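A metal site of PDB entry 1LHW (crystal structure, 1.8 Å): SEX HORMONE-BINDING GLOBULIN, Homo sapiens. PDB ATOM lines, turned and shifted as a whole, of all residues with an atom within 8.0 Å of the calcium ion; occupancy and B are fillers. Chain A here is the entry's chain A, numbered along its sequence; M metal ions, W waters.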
ATOM      1  N   SER A  19      -1.997   9.822 -26.800  1.00  0.00           N
ATOM      2  CA  SER A  19      -2.337  10.355 -28.103  1.00  0.00           C
ATOM      3  C   SER A  19      -1.773   9.430 -29.166  1.00  0.00           C
ATOM      4  O   SER A  19      -0.798   8.712 -28.942  1.00  0.00           O
ATOM      5  CB  SER A  19      -1.766  11.769 -28.293  1.00  0.00           C
ATOM      6  OG  SER A  19      -0.398  11.820 -27.918  1.00  0.00           O
ATOM      7  N   THR A  48       3.397  13.833 -18.227  1.00  0.00           N
ATOM      8  CA  THR A  48       3.420  14.584 -19.475  1.00  0.00           C
ATOM      9  C   THR A  48       4.145  15.925 -19.323  1.00  0.00           C
ATOM     10  O   THR A  48       4.280  16.426 -18.210  1.00  0.00           O
ATOM     11  CB  THR A  48       1.959  14.890 -19.886  1.00  0.00           C
ATOM     12  OG1 THR A  48       1.935  15.594 -21.124  1.00  0.00           O
ATOM     13  CG2 THR A  48       1.286  15.752 -18.806  1.00  0.00           C
ATOM     14  N   TRP A  49       4.612  16.470 -20.456  1.00  0.00           N
ATOM     15  CA  TRP A  49       5.251  17.794 -20.515  1.00  0.00           C
ATOM     16  C   TRP A  49       4.302  18.692 -21.334  1.00  0.00           C
ATOM     17  O   TRP A  49       4.613  19.860 -21.643  1.00  0.00           O
ATOM     18  CB  TRP A  49       6.605  17.750 -21.251  1.00  0.00           C
ATOM     19  CG  TRP A  49       7.686  16.967 -20.550  1.00  0.00           C
ATOM     20  CD1 TRP A  49       8.068  15.673 -20.809  1.00  0.00           C
ATOM     21  CD2 TRP A  49       8.470  17.389 -19.426  1.00  0.00           C
ATOM     22  NE1 TRP A  49       9.036  15.273 -19.921  1.00  0.00           N
ATOM     23  CE2 TRP A  49       9.300  16.306 -19.060  1.00  0.00           C
ATOM     24  CE3 TRP A  49       8.546  18.583 -18.698  1.00  0.00           C
ATOM     25  CZ2 TRP A  49      10.190  16.380 -17.996  1.00  0.00           C
ATOM     26  CZ3 TRP A  49       9.443  18.642 -17.632  1.00  0.00           C
ATOM     27  CH2 TRP A  49      10.251  17.552 -17.294  1.00  0.00           C
ATOM     28  N   ASP A  50       3.146  18.147 -21.697  1.00  0.00           N
ATOM     29  CA  ASP A  50       2.159  18.847 -22.514  1.00  0.00           C
ATOM     30  C   ASP A  50       1.251  19.683 -21.590  1.00  0.00           C
ATOM     31  O   ASP A  50       0.622  19.144 -20.709  1.00  0.00           O
ATOM     32  CB  ASP A  50       1.337  17.798 -23.282  1.00  0.00           C
ATOM     33  CG  ASP A  50       0.504  18.388 -24.412  1.00  0.00           C
ATOM     34  OD1 ASP A  50       0.237  19.616 -24.407  1.00  0.00           O
ATOM     35  OD2 ASP A  50       0.111  17.622 -25.314  1.00  0.00           O
ATOM     36  N   PRO A  51       1.179  21.010 -21.802  1.00  0.00           N
ATOM     37  CA  PRO A  51       0.324  21.811 -20.912  1.00  0.00           C
ATOM     38  C   PRO A  51      -1.167  21.826 -21.258  1.00  0.00           C
ATOM     39  O   PRO A  51      -1.971  22.369 -20.490  1.00  0.00           O
ATOM     40  CB  PRO A  51       0.926  23.219 -21.048  1.00  0.00           C
ATOM     41  CG  PRO A  51       1.302  23.257 -22.515  1.00  0.00           C
ATOM     42  CD  PRO A  51       1.904  21.864 -22.760  1.00  0.00           C
ATOM     43  N   GLU A  52      -1.553  21.241 -22.394  1.00  0.00           N
ATOM     44  CA  GLU A  52      -2.966  21.281 -22.802  1.00  0.00           C
ATOM     45  C   GLU A  52      -3.433  20.034 -23.528  1.00  0.00           C
ATOM     46  O   GLU A  52      -2.739  19.493 -24.397  1.00  0.00           O
ATOM     47  CB  GLU A  52      -3.207  22.491 -23.720  1.00  0.00           C
ATOM     48  CG  GLU A  52      -4.679  22.717 -24.163  1.00  0.00           C
ATOM     49  CD  GLU A  52      -4.908  24.001 -24.979  1.00  0.00           C
ATOM     50  OE1 GLU A  52      -4.483  25.109 -24.537  1.00  0.00           O
ATOM     51  OE2 GLU A  52      -5.560  23.937 -26.046  1.00  0.00           O
ATOM     52  N   GLY A  53      -4.626  19.577 -23.185  1.00  0.00           N
ATOM     53  CA  GLY A  53      -5.144  18.414 -23.862  1.00  0.00           C
ATOM     54  C   GLY A  53      -6.188  17.718 -23.020  1.00  0.00           C
ATOM     55  O   GLY A  53      -6.401  18.050 -21.852  1.00  0.00           O
ATOM     56  N   VAL A  54      -6.827  16.721 -23.629  1.00  0.00           N
ATOM     57  CA  VAL A  54      -7.847  15.973 -22.910  1.00  0.00           C
ATOM     58  C   VAL A  54      -7.282  14.710 -22.285  1.00  0.00           C
ATOM     59  O   VAL A  54      -6.603  13.948 -22.970  1.00  0.00           O
ATOM     60  CB  VAL A  54      -8.981  15.521 -23.867  1.00  0.00           C
ATOM     61  CG1 VAL A  54      -9.983  14.594 -23.091  1.00  0.00           C
ATOM     62  CG2 VAL A  54      -9.652  16.728 -24.479  1.00  0.00           C
ATOM     63  N   LEU A  71      -6.063  19.153 -19.317  1.00  0.00           N
ATOM     64  CA  LEU A  71      -5.088  20.100 -18.829  1.00  0.00           C
ATOM     65  C   LEU A  71      -5.198  21.384 -19.634  1.00  0.00           C
ATOM     66  O   LEU A  71      -5.490  21.351 -20.840  1.00  0.00           O
ATOM     67  CB  LEU A  71      -3.666  19.561 -18.966  1.00  0.00           C
ATOM     68  CG  LEU A  71      -3.244  18.356 -18.103  1.00  0.00           C
ATOM     69  CD1 LEU A  71      -1.749  18.150 -18.286  1.00  0.00           C
ATOM     70  CD2 LEU A  71      -3.585  18.593 -16.621  1.00  0.00           C
ATOM     71  N   VAL A 158      -7.305  22.385 -27.572  1.00  0.00           N
ATOM     72  CA  VAL A 158      -6.798  21.425 -28.573  1.00  0.00           C
ATOM     73  C   VAL A 158      -6.633  20.142 -27.765  1.00  0.00           C
ATOM     74  O   VAL A 158      -5.746  20.020 -26.925  1.00  0.00           O
ATOM     75  CB  VAL A 158      -5.453  21.905 -29.164  1.00  0.00           C
ATOM     76  CG1 VAL A 158      -4.946  20.902 -30.209  1.00  0.00           C
ATOM     77  CG2 VAL A 158      -5.652  23.252 -29.798  1.00  0.00           C
ATOM     78  N   PRO A 159      -7.494  19.136 -28.039  1.00  0.00           N
ATOM     79  CA  PRO A 159      -7.476  17.851 -27.326  1.00  0.00           C
ATOM     80  C   PRO A 159      -6.221  17.006 -27.206  1.00  0.00           C
ATOM     81  O   PRO A 159      -6.028  16.341 -26.198  1.00  0.00           O
ATOM     82  CB  PRO A 159      -8.655  17.093 -27.974  1.00  0.00           C
ATOM     83  CG  PRO A 159      -8.623  17.569 -29.381  1.00  0.00           C
ATOM     84  CD  PRO A 159      -8.345  19.074 -29.234  1.00  0.00           C
ATOM     85  N   ALA A 160      -5.347  17.027 -28.205  1.00  0.00           N
ATOM     86  CA  ALA A 160      -4.159  16.184 -28.132  1.00  0.00           C
ATOM     87  C   ALA A 160      -3.332  16.388 -26.875  1.00  0.00           C
ATOM     88  O   ALA A 160      -2.832  17.478 -26.605  1.00  0.00           O
ATOM     89  CB  ALA A 160      -3.257  16.406 -29.376  1.00  0.00           C
ATOM     90  N   LEU A 161      -3.180  15.306 -26.125  1.00  0.00           N
ATOM     91  CA  LEU A 161      -2.381  15.343 -24.927  1.00  0.00           C
ATOM     92  C   LEU A 161      -1.259  14.325 -25.076  1.00  0.00           C
ATOM     93  O   LEU A 161      -1.483  13.114 -25.047  1.00  0.00           O
ATOM     94  CB  LEU A 161      -3.200  15.012 -23.690  1.00  0.00           C
ATOM     95  CG  LEU A 161      -2.379  15.184 -22.408  1.00  0.00           C
ATOM     96  CD1 LEU A 161      -2.058  16.666 -22.243  1.00  0.00           C
ATOM     97  CD2 LEU A 161      -3.140  14.658 -21.209  1.00  0.00           C
ATOM     98  N   ASP A 162      -0.053  14.849 -25.246  1.00  0.00           N
ATOM     99  CA  ASP A 162       1.142  14.037 -25.419  1.00  0.00           C
ATOM    100  C   ASP A 162       1.619  13.591 -24.039  1.00  0.00           C
ATOM    101  O   ASP A 162       2.491  14.210 -23.439  1.00  0.00           O
ATOM    102  CB  ASP A 162       2.225  14.889 -26.110  1.00  0.00           C
ATOM    103  CG  ASP A 162       3.426  14.074 -26.542  1.00  0.00           C
ATOM    104  OD1 ASP A 162       3.371  12.828 -26.460  1.00  0.00           O
ATOM    105  OD2 ASP A 162       4.440  14.681 -26.967  1.00  0.00           O
ATOM    106  N   GLY A 163       1.027  12.519 -23.536  1.00  0.00           N
ATOM    107  CA  GLY A 163       1.397  12.039 -22.228  1.00  0.00           C
ATOM    108  C   GLY A 163       1.193  10.550 -22.116  1.00  0.00           C
ATOM    109  O   GLY A 163       0.769   9.906 -23.072  1.00  0.00           O
HETATM  110 CA    CA M   1      -1.396  19.159 -26.206  1.00  0.00          CA
HETATM  111  O   HOH W   1      -0.199  18.564 -28.050  1.00  0.00           O
HETATM  112  O   HOH W   2      -0.396  21.456 -26.497  1.00  0.00           O
HETATM  113  O   HOH W   3      -3.082  20.425 -27.332  1.00  0.00           O
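N of Asp 162 sits close to OD2 of Asp 50 (2.8 Å). N of Asp 50 lies within hydrogen-bond range of OG1 of Thr 48, at 2.9 Å. The side-chain carboxylate of Glu 52 sits at hydrogen-bond distance from the backbone NH of Val 158 (2.8 Å).
Within 4 Å of the calcium ion: Asp 50, Glu 52 and Ala 160.
The calcium ion is bound by the backbone carbonyl oxygen (O) of Ala 160 (2.2 Å), water W1 (2.3 Å), the backbone carbonyl oxygen (O) of Glu 52 (2.3 Å), the side-chain carboxylate (OD2) of Asp 50 (2.3 Å), water W3 (2.4 Å), the side-chain carboxylate (OD1) of Asp 50 (2.5 Å) and water W2 (2.5 Å). The calcium ion has seven donor atoms within binding distance.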
